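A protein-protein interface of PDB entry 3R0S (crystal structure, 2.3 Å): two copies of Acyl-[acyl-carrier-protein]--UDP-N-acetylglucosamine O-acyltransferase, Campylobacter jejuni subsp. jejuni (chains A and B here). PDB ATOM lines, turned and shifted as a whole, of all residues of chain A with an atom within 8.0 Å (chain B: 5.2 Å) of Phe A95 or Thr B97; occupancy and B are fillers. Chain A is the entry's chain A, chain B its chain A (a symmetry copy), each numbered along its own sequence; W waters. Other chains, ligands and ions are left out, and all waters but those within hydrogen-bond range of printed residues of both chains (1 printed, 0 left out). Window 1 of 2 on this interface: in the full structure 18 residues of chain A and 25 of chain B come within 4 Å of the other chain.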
ATOM      1  N   GLN A  45      13.261  -8.556  -9.936  1.00  0.00           N
ATOM      2  CA  GLN A  45      14.321  -8.548 -10.888  1.00  0.00           C
ATOM      3  C   GLN A  45      14.045  -9.525 -12.004  1.00  0.00           C
ATOM      4  O   GLN A  45      13.782 -10.721 -11.784  1.00  0.00           O
ATOM      5  CB  GLN A  45      15.629  -8.918 -10.203  1.00  0.00           C
ATOM      6  CG  GLN A  45      16.740  -9.152 -11.177  1.00  0.00           C
ATOM      7  CD  GLN A  45      18.091  -9.215 -10.511  1.00  0.00           C
ATOM      8  OE1 GLN A  45      18.245  -8.777  -9.385  1.00  0.00           O
ATOM      9  NE2 GLN A  45      19.085  -9.740 -11.217  1.00  0.00           N
ATOM     10  N   ALA A  47      11.707  -9.936 -14.218  1.00  0.00           N
ATOM     11  CA  ALA A  47      10.406 -10.323 -14.657  1.00  0.00           C
ATOM     12  C   ALA A  47      10.037  -9.430 -15.822  1.00  0.00           C
ATOM     13  O   ALA A  47      10.516  -8.270 -15.923  1.00  0.00           O
ATOM     14  CB  ALA A  47       9.394 -10.158 -13.526  1.00  0.00           C
ATOM     15  N   VAL A  61       4.936  -9.730  -8.701  1.00  0.00           N
ATOM     16  CA  VAL A  61       5.524 -10.559  -9.701  1.00  0.00           C
ATOM     17  C   VAL A  61       6.981 -10.792  -9.365  1.00  0.00           C
ATOM     18  O   VAL A  61       7.778  -9.846  -9.248  1.00  0.00           O
ATOM     19  CB  VAL A  61       5.340  -9.912 -11.068  1.00  0.00           C
ATOM     20  CG1 VAL A  61       5.820 -10.804 -12.186  1.00  0.00           C
ATOM     21  CG2 VAL A  61       3.836  -9.542 -11.280  1.00  0.00           C
ATOM     22  N   PHE A  62       7.319 -12.056  -9.154  1.00  0.00           N
ATOM     23  CA  PHE A  62       8.581 -12.454  -8.590  1.00  0.00           C
ATOM     24  C   PHE A  62       9.637 -12.637  -9.647  1.00  0.00           C
ATOM     25  O   PHE A  62       9.370 -12.453 -10.822  1.00  0.00           O
ATOM     26  CB  PHE A  62       8.387 -13.704  -7.745  1.00  0.00           C
ATOM     27  CG  PHE A  62       7.911 -13.419  -6.307  1.00  0.00           C
ATOM     28  CD1 PHE A  62       6.678 -12.889  -6.064  1.00  0.00           C
ATOM     29  CD2 PHE A  62       8.736 -13.681  -5.232  1.00  0.00           C
ATOM     30  CE1 PHE A  62       6.210 -12.655  -4.740  1.00  0.00           C
ATOM     31  CE2 PHE A  62       8.338 -13.437  -3.907  1.00  0.00           C
ATOM     32  CZ  PHE A  62       7.054 -12.914  -3.659  1.00  0.00           C
ATOM     33  N   SER A  63      10.859 -12.965  -9.241  1.00  0.00           N
ATOM     34  CA  SER A  63      11.981 -12.852 -10.154  1.00  0.00           C
ATOM     35  C   SER A  63      11.760 -13.720 -11.363  1.00  0.00           C
ATOM     36  O   SER A  63      11.537 -14.893 -11.232  1.00  0.00           O
ATOM     37  CB  SER A  63      13.299 -13.299  -9.517  1.00  0.00           C
ATOM     38  OG  SER A  63      13.519 -12.704  -8.274  1.00  0.00           O
ATOM     39  N   TYR A  64      11.915 -13.126 -12.529  1.00  0.00           N
ATOM     40  CA  TYR A  64      11.964 -13.832 -13.826  1.00  0.00           C
ATOM     41  C   TYR A  64      10.617 -14.391 -14.360  1.00  0.00           C
ATOM     42  O   TYR A  64      10.631 -15.029 -15.376  1.00  0.00           O
ATOM     43  CB  TYR A  64      13.029 -14.912 -13.815  1.00  0.00           C
ATOM     44  CG  TYR A  64      14.363 -14.316 -13.488  1.00  0.00           C
ATOM     45  CD1 TYR A  64      14.945 -13.409 -14.344  1.00  0.00           C
ATOM     46  CD2 TYR A  64      15.048 -14.646 -12.310  1.00  0.00           C
ATOM     47  CE1 TYR A  64      16.166 -12.824 -14.055  1.00  0.00           C
ATOM     48  CE2 TYR A  64      16.278 -14.086 -12.023  1.00  0.00           C
ATOM     49  CZ  TYR A  64      16.828 -13.152 -12.896  1.00  0.00           C
ATOM     50  OH  TYR A  64      18.041 -12.533 -12.630  1.00  0.00           O
ATOM     51  N   ALA A  65       9.505 -14.088 -13.696  1.00  0.00           N
ATOM     52  CA  ALA A  65       8.197 -14.478 -14.159  1.00  0.00           C
ATOM     53  C   ALA A  65       7.897 -13.682 -15.406  1.00  0.00           C
ATOM     54  O   ALA A  65       8.281 -12.518 -15.506  1.00  0.00           O
ATOM     55  CB  ALA A  65       7.106 -14.247 -13.056  1.00  0.00           C
ATOM     56  N   ILE A  66       7.246 -14.343 -16.371  1.00  0.00           N
ATOM     57  CA  ILE A  66       6.978 -13.827 -17.718  1.00  0.00           C
ATOM     58  C   ILE A  66       5.473 -13.832 -17.883  1.00  0.00           C
ATOM     59  O   ILE A  66       4.870 -14.924 -17.819  1.00  0.00           O
ATOM     60  CB  ILE A  66       7.573 -14.758 -18.814  1.00  0.00           C
ATOM     61  CG1 ILE A  66       9.073 -15.083 -18.570  1.00  0.00           C
ATOM     62  CG2 ILE A  66       7.380 -14.168 -20.217  1.00  0.00           C
ATOM     63  CD1 ILE A  66      10.051 -13.882 -18.436  1.00  0.00           C
ATOM     64  N   ILE A  92       2.588 -13.940  -8.283  1.00  0.00           N
ATOM     65  CA  ILE A  92       3.123 -14.770  -9.314  1.00  0.00           C
ATOM     66  C   ILE A  92       4.595 -15.002  -8.976  1.00  0.00           C
ATOM     67  O   ILE A  92       5.435 -14.065  -9.056  1.00  0.00           O
ATOM     68  CB  ILE A  92       2.896 -14.114 -10.627  1.00  0.00           C
ATOM     69  CG1 ILE A  92       1.376 -13.877 -10.786  1.00  0.00           C
ATOM     70  CG2 ILE A  92       3.443 -14.920 -11.765  1.00  0.00           C
ATOM     71  CD1 ILE A  92       0.997 -12.962 -11.789  1.00  0.00           C
ATOM     72  N   ARG A  93       4.878 -16.261  -8.603  1.00  0.00           N
ATOM     73  CA  ARG A  93       6.159 -16.695  -8.209  1.00  0.00           C
ATOM     74  C   ARG A  93       7.069 -16.902  -9.404  1.00  0.00           C
ATOM     75  O   ARG A  93       6.664 -16.727 -10.540  1.00  0.00           O
ATOM     76  CB  ARG A  93       6.067 -17.964  -7.317  1.00  0.00           C
ATOM     77  CG  ARG A  93       5.372 -17.675  -5.964  1.00  0.00           C
ATOM     78  CD  ARG A  93       6.051 -16.511  -5.147  1.00  0.00           C
ATOM     79  NE  ARG A  93       7.447 -16.815  -4.821  1.00  0.00           N
ATOM     80  CZ  ARG A  93       7.985 -16.980  -3.601  1.00  0.00           C
ATOM     81  NH1 ARG A  93       7.306 -16.811  -2.453  1.00  0.00           N
ATOM     82  NH2 ARG A  93       9.266 -17.252  -3.526  1.00  0.00           N
ATOM     83  N   GLU A  94       8.313 -17.267  -9.108  1.00  0.00           N
ATOM     84  CA  GLU A  94       9.384 -17.238 -10.075  1.00  0.00           C
ATOM     85  C   GLU A  94       9.205 -18.164 -11.254  1.00  0.00           C
ATOM     86  O   GLU A  94       8.766 -19.305 -11.092  1.00  0.00           O
ATOM     87  CB  GLU A  94      10.702 -17.586  -9.388  1.00  0.00           C
ATOM     88  CG  GLU A  94      11.137 -16.528  -8.313  1.00  0.00           C
ATOM     89  CD  GLU A  94      10.588 -16.764  -6.861  1.00  0.00           C
ATOM     90  OE1 GLU A  94       9.496 -17.360  -6.698  1.00  0.00           O
ATOM     91  OE2 GLU A  94      11.280 -16.362  -5.875  1.00  0.00           O
ATOM     92  N   PHE A  95       9.623 -17.690 -12.434  1.00  0.00           N
ATOM     93  CA  PHE A  95       9.663 -18.507 -13.654  1.00  0.00           C
ATOM     94  C   PHE A  95       8.274 -18.938 -14.223  1.00  0.00           C
ATOM     95  O   PHE A  95       8.188 -19.813 -15.063  1.00  0.00           O
ATOM     96  CB  PHE A  95      10.565 -19.677 -13.477  1.00  0.00           C
ATOM     97  CG  PHE A  95      11.880 -19.310 -12.830  1.00  0.00           C
ATOM     98  CD1 PHE A  95      12.714 -18.401 -13.408  1.00  0.00           C
ATOM     99  CD2 PHE A  95      12.273 -19.886 -11.619  1.00  0.00           C
ATOM    100  CE1 PHE A  95      13.914 -18.058 -12.782  1.00  0.00           C
ATOM    101  CE2 PHE A  95      13.431 -19.517 -10.993  1.00  0.00           C
ATOM    102  CZ  PHE A  95      14.264 -18.654 -11.566  1.00  0.00           C
ATOM    103  N   ALA A  96       7.228 -18.271 -13.796  1.00  0.00           N
ATOM    104  CA  ALA A  96       5.891 -18.582 -14.276  1.00  0.00           C
ATOM    105  C   ALA A  96       5.759 -18.050 -15.662  1.00  0.00           C
ATOM    106  O   ALA A  96       6.358 -17.016 -15.959  1.00  0.00           O
ATOM    107  CB  ALA A  96       4.887 -17.951 -13.408  1.00  0.00           C
ATOM    108  N   THR A  97       5.008 -18.751 -16.511  1.00  0.00           N
ATOM    109  CA  THR A  97       4.814 -18.361 -17.888  1.00  0.00           C
ATOM    110  C   THR A  97       3.299 -18.263 -18.105  1.00  0.00           C
ATOM    111  O   THR A  97       2.594 -19.290 -18.137  1.00  0.00           O
ATOM    112  CB  THR A  97       5.472 -19.347 -18.868  1.00  0.00           C
ATOM    113  OG1 THR A  97       5.181 -20.708 -18.498  1.00  0.00           O
ATOM    114  CG2 THR A  97       7.038 -19.193 -18.909  1.00  0.00           C
ATOM    115  N   ILE A  98       2.793 -17.033 -18.172  1.00  0.00           N
ATOM    116  CA  ILE A  98       1.398 -16.740 -18.475  1.00  0.00           C
ATOM    117  C   ILE A  98       1.293 -16.076 -19.863  1.00  0.00           C
ATOM    118  O   ILE A  98       1.646 -14.925 -20.045  1.00  0.00           O
ATOM    119  CB  ILE A  98       0.834 -15.866 -17.404  1.00  0.00           C
ATOM    120  CG1 ILE A  98       1.174 -16.472 -16.033  1.00  0.00           C
ATOM    121  CG2 ILE A  98      -0.689 -15.690 -17.574  1.00  0.00           C
ATOM    122  CD1 ILE A  98       0.439 -15.763 -14.850  1.00  0.00           C
ATOM    123  N   ILE A 117       0.014 -18.064  -7.589  1.00  0.00           N
ATOM    124  CA  ILE A 117       0.595 -18.883  -8.649  1.00  0.00           C
ATOM    125  C   ILE A 117       2.078 -19.094  -8.341  1.00  0.00           C
ATOM    126  O   ILE A 117       2.874 -18.130  -8.371  1.00  0.00           O
ATOM    127  CB  ILE A 117       0.445 -18.171  -9.967  1.00  0.00           C
ATOM    128  CG1 ILE A 117      -1.042 -18.059 -10.300  1.00  0.00           C
ATOM    129  CG2 ILE A 117       1.228 -18.878 -11.187  1.00  0.00           C
ATOM    130  CD1 ILE A 117      -1.301 -17.146 -11.446  1.00  0.00           C
ATOM    131  N   MET A 118       2.425 -20.350  -8.013  1.00  0.00           N
ATOM    132  CA  MET A 118       3.708 -20.705  -7.505  1.00  0.00           C
ATOM    133  C   MET A 118       4.696 -20.929  -8.629  1.00  0.00           C
ATOM    134  O   MET A 118       4.393 -20.753  -9.798  1.00  0.00           O
ATOM    135  CB  MET A 118       3.599 -21.935  -6.599  1.00  0.00           C
ATOM    136  CG  MET A 118       2.769 -21.701  -5.355  1.00  0.00           C
ATOM    137  SD  MET A 118       2.781 -23.135  -4.110  1.00  0.00           S
ATOM    138  CE  MET A 118       0.929 -22.879  -3.624  1.00  0.00           C
ATOM    139  N   ALA A 119       5.903 -21.298  -8.269  1.00  0.00           N
ATOM    140  CA  ALA A 119       7.023 -21.267  -9.241  1.00  0.00           C
ATOM    141  C   ALA A 119       6.807 -22.267 -10.363  1.00  0.00           C
ATOM    142  O   ALA A 119       6.244 -23.342 -10.130  1.00  0.00           O
ATOM    143  CB  ALA A 119       8.393 -21.563  -8.532  1.00  0.00           C
ATOM    144  N   TYR A 120       7.292 -21.884 -11.549  1.00  0.00           N
ATOM    145  CA  TYR A 120       7.275 -22.681 -12.776  1.00  0.00           C
ATOM    146  C   TYR A 120       5.858 -22.959 -13.317  1.00  0.00           C
ATOM    147  O   TYR A 120       5.694 -23.763 -14.191  1.00  0.00           O
ATOM    148  CB  TYR A 120       8.012 -24.003 -12.595  1.00  0.00           C
ATOM    149  CG  TYR A 120       9.255 -23.939 -11.743  1.00  0.00           C
ATOM    150  CD1 TYR A 120      10.463 -23.437 -12.232  1.00  0.00           C
ATOM    151  CD2 TYR A 120       9.273 -24.493 -10.449  1.00  0.00           C
ATOM    152  CE1 TYR A 120      11.586 -23.422 -11.443  1.00  0.00           C
ATOM    153  CE2 TYR A 120      10.406 -24.464  -9.671  1.00  0.00           C
ATOM    154  CZ  TYR A 120      11.560 -23.888 -10.160  1.00  0.00           C
ATOM    155  OH  TYR A 120      12.705 -23.892  -9.371  1.00  0.00           O
ATOM    156  N   CYS A 121       4.845 -22.296 -12.799  1.00  0.00           N
ATOM    157  CA  CYS A 121       3.501 -22.528 -13.256  1.00  0.00           C
ATOM    158  C   CYS A 121       3.288 -21.953 -14.635  1.00  0.00           C
ATOM    159  O   CYS A 121       3.816 -20.887 -14.962  1.00  0.00           O
ATOM    160  CB  CYS A 121       2.479 -21.943 -12.295  1.00  0.00           C
ATOM    161  SG  CYS A 121       2.183 -22.911 -10.788  1.00  0.00           S
ATOM    162  N   HIS A 122       2.509 -22.674 -15.447  1.00  0.00           N
ATOM    163  CA  HIS A 122       2.252 -22.303 -16.791  1.00  0.00           C
ATOM    164  C   HIS A 122       0.768 -22.178 -17.027  1.00  0.00           C
ATOM    165  O   HIS A 122      -0.011 -23.130 -16.781  1.00  0.00           O
ATOM    166  CB  HIS A 122       2.814 -23.358 -17.710  1.00  0.00           C
ATOM    167  CG  HIS A 122       2.551 -23.082 -19.144  1.00  0.00           C
ATOM    168  ND1 HIS A 122       3.202 -22.085 -19.840  1.00  0.00           N
ATOM    169  CD2 HIS A 122       1.692 -23.662 -20.024  1.00  0.00           C
ATOM    170  CE1 HIS A 122       2.756 -22.065 -21.086  1.00  0.00           C
ATOM    171  NE2 HIS A 122       1.842 -23.013 -21.226  1.00  0.00           N
ATOM    172  N   ASN A 137       3.404 -25.579  -7.449  1.00  0.00           N
ATOM    173  CA  ASN A 137       4.557 -25.611  -8.361  1.00  0.00           C
ATOM    174  C   ASN A 137       4.341 -26.510  -9.577  1.00  0.00           C
ATOM    175  O   ASN A 137       3.841 -27.633  -9.433  1.00  0.00           O
ATOM    176  CB  ASN A 137       5.818 -26.074  -7.650  1.00  0.00           C
ATOM    177  CG  ASN A 137       6.127 -25.245  -6.418  1.00  0.00           C
ATOM    178  OD1 ASN A 137       6.531 -24.131  -6.517  1.00  0.00           O
ATOM    179  ND2 ASN A 137       5.878 -25.808  -5.250  1.00  0.00           N
ATOM    180  N   ASN A 138       4.681 -25.973 -10.754  1.00  0.00           N
ATOM    181  CA  ASN A 138       4.582 -26.632 -12.016  1.00  0.00           C
ATOM    182  C   ASN A 138       3.162 -27.049 -12.492  1.00  0.00           C
ATOM    183  O   ASN A 138       3.058 -27.756 -13.422  1.00  0.00           O
ATOM    184  CB  ASN A 138       5.440 -27.868 -12.031  1.00  0.00           C
ATOM    185  CG  ASN A 138       6.889 -27.616 -11.621  1.00  0.00           C
ATOM    186  OD1 ASN A 138       7.245 -27.917 -10.486  1.00  0.00           O
ATOM    187  ND2 ASN A 138       7.755 -27.160 -12.578  1.00  0.00           N
ATOM    188  N   TYR B  64      20.437 -17.899 -13.115  1.00  0.00           N
ATOM    189  CA  TYR B  64      19.044 -17.600 -12.723  1.00  0.00           C
ATOM    190  C   TYR B  64      18.487 -18.378 -11.500  1.00  0.00           C
ATOM    191  O   TYR B  64      17.339 -18.211 -11.197  1.00  0.00           O
ATOM    192  CB  TYR B  64      18.108 -17.726 -13.911  1.00  0.00           C
ATOM    193  CG  TYR B  64      18.554 -16.817 -15.014  1.00  0.00           C
ATOM    194  CD1 TYR B  64      18.538 -15.452 -14.836  1.00  0.00           C
ATOM    195  CD2 TYR B  64      19.007 -17.317 -16.244  1.00  0.00           C
ATOM    196  CE1 TYR B  64      18.966 -14.588 -15.830  1.00  0.00           C
ATOM    197  CE2 TYR B  64      19.415 -16.464 -17.251  1.00  0.00           C
ATOM    198  CZ  TYR B  64      19.412 -15.089 -17.030  1.00  0.00           C
ATOM    199  OH  TYR B  64      19.851 -14.196 -17.997  1.00  0.00           O
ATOM    200  N   ALA B  65      19.326 -19.148 -10.812  1.00  0.00           N
ATOM    201  CA  ALA B  65      18.934 -19.836  -9.608  1.00  0.00           C
ATOM    202  C   ALA B  65      18.710 -18.796  -8.538  1.00  0.00           C
ATOM    203  O   ALA B  65      19.422 -17.794  -8.489  1.00  0.00           O
ATOM    204  CB  ALA B  65      20.014 -20.886  -9.169  1.00  0.00           C
ATOM    205  N   ILE B  66      17.681 -19.027  -7.713  1.00  0.00           N
ATOM    206  CA  ILE B  66      17.184 -18.092  -6.699  1.00  0.00           C
ATOM    207  C   ILE B  66      17.301 -18.806  -5.368  1.00  0.00           C
ATOM    208  O   ILE B  66      16.650 -19.858  -5.198  1.00  0.00           O
ATOM    209  CB  ILE B  66      15.681 -17.757  -6.920  1.00  0.00           C
ATOM    210  CG1 ILE B  66      15.379 -17.299  -8.374  1.00  0.00           C
ATOM    211  CG2 ILE B  66      15.186 -16.703  -5.920  1.00  0.00           C
ATOM    212  CD1 ILE B  66      16.185 -16.087  -8.922  1.00  0.00           C
ATOM    213  N   ASP B  69      14.654 -16.490  -1.428  1.00  0.00           N
ATOM    214  CA  ASP B  69      13.341 -15.887  -1.635  1.00  0.00           C
ATOM    215  C   ASP B  69      12.430 -16.255  -0.492  1.00  0.00           C
ATOM    216  O   ASP B  69      12.652 -17.236   0.195  1.00  0.00           O
ATOM    217  CB  ASP B  69      12.654 -16.256  -2.990  1.00  0.00           C
ATOM    218  CG  ASP B  69      12.864 -17.769  -3.453  1.00  0.00           C
ATOM    219  OD1 ASP B  69      13.789 -18.472  -2.977  1.00  0.00           O
ATOM    220  OD2 ASP B  69      12.107 -18.213  -4.386  1.00  0.00           O
ATOM    221  N   PHE B  95      17.566 -22.081 -12.510  1.00  0.00           N
ATOM    222  CA  PHE B  95      16.147 -21.901 -12.180  1.00  0.00           C
ATOM    223  C   PHE B  95      15.666 -22.600 -10.869  1.00  0.00           C
ATOM    224  O   PHE B  95      14.480 -22.736 -10.632  1.00  0.00           O
ATOM    225  CB  PHE B  95      15.285 -22.262 -13.337  1.00  0.00           C
ATOM    226  CG  PHE B  95      15.784 -21.687 -14.641  1.00  0.00           C
ATOM    227  CD1 PHE B  95      15.919 -20.341 -14.806  1.00  0.00           C
ATOM    228  CD2 PHE B  95      16.127 -22.519 -15.711  1.00  0.00           C
ATOM    229  CE1 PHE B  95      16.405 -19.832 -16.012  1.00  0.00           C
ATOM    230  CE2 PHE B  95      16.638 -22.014 -16.876  1.00  0.00           C
ATOM    231  CZ  PHE B  95      16.744 -20.702 -17.054  1.00  0.00           C
ATOM    232  N   ALA B  96      16.596 -22.971 -10.021  1.00  0.00           N
ATOM    233  CA  ALA B  96      16.254 -23.614  -8.763  1.00  0.00           C
ATOM    234  C   ALA B  96      15.720 -22.575  -7.838  1.00  0.00           C
ATOM    235  O   ALA B  96      16.171 -21.432  -7.909  1.00  0.00           O
ATOM    236  CB  ALA B  96      17.450 -24.232  -8.173  1.00  0.00           C
ATOM    237  N   THR B  97      14.757 -22.950  -6.997  1.00  0.00           N
ATOM    238  CA  THR B  97      14.136 -22.039  -6.064  1.00  0.00           C
ATOM    239  C   THR B  97      14.293 -22.664  -4.672  1.00  0.00           C
ATOM    240  O   THR B  97      13.641 -23.677  -4.353  1.00  0.00           O
ATOM    241  CB  THR B  97      12.661 -21.770  -6.409  1.00  0.00           C
ATOM    242  OG1 THR B  97      11.977 -22.998  -6.720  1.00  0.00           O
ATOM    243  CG2 THR B  97      12.504 -20.813  -7.649  1.00  0.00           C
ATOM    244  N   ILE B  98      15.213 -22.114  -3.881  1.00  0.00           N
ATOM    245  CA  ILE B  98      15.433 -22.503  -2.494  1.00  0.00           C
ATOM    246  C   ILE B  98      14.990 -21.363  -1.554  1.00  0.00           C
ATOM    247  O   ILE B  98      15.642 -20.341  -1.444  1.00  0.00           O
ATOM    248  CB  ILE B  98      16.875 -22.843  -2.301  1.00  0.00           C
ATOM    249  CG1 ILE B  98      17.313 -23.811  -3.413  1.00  0.00           C
ATOM    250  CG2 ILE B  98      17.121 -23.449  -0.905  1.00  0.00           C
ATOM    251  CD1 ILE B  98      18.737 -24.410  -3.178  1.00  0.00           C
ATOM    252  N   ASN B  99      13.822 -21.540  -0.946  1.00  0.00           N
ATOM    253  CA  ASN B  99      13.151 -20.505  -0.204  1.00  0.00           C
ATOM    254  C   ASN B  99      13.634 -20.482   1.249  1.00  0.00           C
ATOM    255  O   ASN B  99      14.097 -21.466   1.769  1.00  0.00           O
ATOM    256  CB  ASN B  99      11.653 -20.755  -0.187  1.00  0.00           C
ATOM    257  CG  ASN B  99      11.027 -20.744  -1.565  1.00  0.00           C
ATOM    258  OD1 ASN B  99       9.912 -21.226  -1.727  1.00  0.00           O
ATOM    259  ND2 ASN B  99      11.694 -20.159  -2.531  1.00  0.00           N
ATOM    260  N   CYS B 121      14.739 -27.360  -9.628  1.00  0.00           N
ATOM    261  CA  CYS B 121      14.470 -27.971  -8.353  1.00  0.00           C
ATOM    262  C   CYS B 121      13.984 -26.951  -7.353  1.00  0.00           C
ATOM    263  O   CYS B 121      14.449 -25.808  -7.340  1.00  0.00           O
ATOM    264  CB  CYS B 121      15.699 -28.678  -7.807  1.00  0.00           C
ATOM    265  SG  CYS B 121      16.066 -30.291  -8.554  1.00  0.00           S
ATOM    266  N   HIS B 122      13.036 -27.374  -6.511  1.00  0.00           N
ATOM    267  CA  HIS B 122      12.434 -26.527  -5.547  1.00  0.00           C
ATOM    268  C   HIS B 122      12.593 -27.107  -4.164  1.00  0.00           C
ATOM    269  O   HIS B 122      12.194 -28.267  -3.897  1.00  0.00           O
ATOM    270  CB  HIS B 122      10.966 -26.386  -5.861  1.00  0.00           C
ATOM    271  CG  HIS B 122      10.235 -25.553  -4.875  1.00  0.00           C
ATOM    272  ND1 HIS B 122      10.382 -24.183  -4.805  1.00  0.00           N
ATOM    273  CD2 HIS B 122       9.355 -25.891  -3.895  1.00  0.00           C
ATOM    274  CE1 HIS B 122       9.622 -23.715  -3.828  1.00  0.00           C
ATOM    275  NE2 HIS B 122       8.986 -24.729  -3.262  1.00  0.00           N
ATOM    276  N   ILE B 123      13.184 -26.304  -3.282  1.00  0.00           N
ATOM    277  CA  ILE B 123      13.288 -26.615  -1.869  1.00  0.00           C
ATOM    278  C   ILE B 123      12.532 -25.550  -1.091  1.00  0.00           C
ATOM    279  O   ILE B 123      12.933 -24.364  -1.101  1.00  0.00           O
ATOM    280  CB  ILE B 123      14.721 -26.627  -1.439  1.00  0.00           C
ATOM    281  CG1 ILE B 123      15.491 -27.706  -2.201  1.00  0.00           C
ATOM    282  CG2 ILE B 123      14.842 -26.844   0.116  1.00  0.00           C
ATOM    283  CD1 ILE B 123      17.041 -27.715  -1.877  1.00  0.00           C
ATOM    284  N   ALA B 124      11.462 -25.990  -0.420  1.00  0.00           N
ATOM    285  CA  ALA B 124      10.551 -25.154   0.314  1.00  0.00           C
ATOM    286  C   ALA B 124      11.051 -24.732   1.677  1.00  0.00           C
ATOM    287  O   ALA B 124      11.988 -25.274   2.211  1.00  0.00           O
ATOM    288  CB  ALA B 124       9.169 -25.863   0.476  1.00  0.00           C
HETATM  289  O   HOH W   1       9.362 -19.949  -5.147  1.00  0.00           O
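The side-chain carboxylate (OD2) of Asp B69 lies within salt-bridge range of the guanidinium group (NH2) of Arg A93 (3.1 Å). The side-chain carboxylate (OE2) of Glu A94 lies close to the side-chain carboxylate (OD2) of Asp B69 (2.5 Å). The backbone carbonyl oxygen of Phe B95 sits at hydrogen-bond distance from the side-chain hydroxyl of Tyr A120 (2.5 Å). The side-chain hydroxyl (OH) of Tyr A120 is in hydrogen-bond range of the side-chain hydroxyl (OG1) of Thr B97 (2.9 Å). The side-chain hydroxyl of Tyr A120 sits at hydrogen-bond distance from the backbone carbonyl oxygen of Cys B121 (3.3 Å).
O of Gln A45 sits at hydrogen-bond distance from N of Tyr A64, at 3.1 Å. The backbone NH (N) of Arg A93 lies within hydrogen-bond range of the backbone carbonyl oxygen (O) of Ile A117. The backbone NH of Tyr A120 lies within hydrogen-bond range of the backbone carbonyl oxygen of Glu A94, at 3.0 Å. The backbone NH of Thr B97 is in hydrogen-bond range of the backbone carbonyl oxygen of Cys B121. N of Ile B123 lies within hydrogen-bond range of O of Thr B97, 2.9 Å away. The backbone carbonyl oxygen (O) of Ile B123 sits at hydrogen-bond distance from the backbone NH (N) of Asn B99 (3.0 Å).
Tyr A64 touches Tyr B64 (CZ to CD1, 3.5 Å). Tyr A64 touches Ile B66. NH2 of Arg A93 touches ND2 of Asn B99, 3.9 Å away. OE2 of Glu A94 touches CG2 of Ile B66, at 3.9 Å. CZ of Phe A95 touches O of Tyr B64, 3.1 Å away. CG1 of Ile B66 touches CZ of Phe A95 (3.6 Å). Phe B95 touches Phe A95. CE2 of Phe A95 touches CG2 of Thr B97, 3.7 Å away. CA of Ala B96 touches OH of Tyr A120, 3.6 Å away. ND2 of Asn A137 touches CD2 of His B122 (3.7 Å).
Printed residues of chain B within 4 Å of Tyr A120: Phe B95, Ala B96, Thr B97 and Cys B121. Asn A138 touches none of the printed residues of chain B. Printed residues of chain A within 4 Å of Ile B66: Tyr A64, Glu A94 and Phe A95. Of the printed residues of chain A, Ala B96 touches Tyr A120. Thr B97 touches just these residues of chain A: Phe A95 (3.7 Å) and Tyr A120 (2.9 Å). Of the printed residues of chain A, His B122 touches Asn A137. The nearest residue of chain A that does not touch Thr B97 is Glu A94 (4.1 Å). The nearest printed residue of chain A that does not touch Tyr B64 is Ser A63 (6.6 Å).
Hydrophobic or aromatic side chains of chain B within 4 Å of the printed part of chain A: Tyr B64, Ile B66, Phe B95 and His B122. Printed residues of chain A that touch a printed residue of chain B: Tyr A64, Arg A93, Glu A94, Phe A95, Tyr A120 and Asn A137. Hydrophobic or aromatic side chains of chain A within 4 Å of the printed part of chain B: Tyr A64, Phe A95 and Tyr A120. Among the printed residues, 15 pairs touch across the chains. Among the printed residues, Asp or Glu carboxylates within 4 Å of a Lys or Arg side-chain nitrogen of the other chain: Arg A93 with Asp B69 (3.1 Å).
Tyr A64 touches its own counterpart, Tyr B64. Tyr A64 touches Ile B66, but with the chains exchanged Ile A66 does not touch Tyr B64 (9.3 Å). Phe A95 touches Tyr B64, but with the chains exchanged Tyr A64 does not touch Phe B95 (6.2 Å). Phe B95 touches its own counterpart, Phe A95. Positions printed for both chains: 64, 65, 66, 95, 96, 97, 98, 121 and 122. Of the 15 pairs that touch across the chains among the printed residues, 2 have their exchanged pair printed and touching as well.
Water W1 lies within hydrogen-bond range of OE1 of Glu A94, NH2 of Arg A93 and OD2 of Asp B69.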
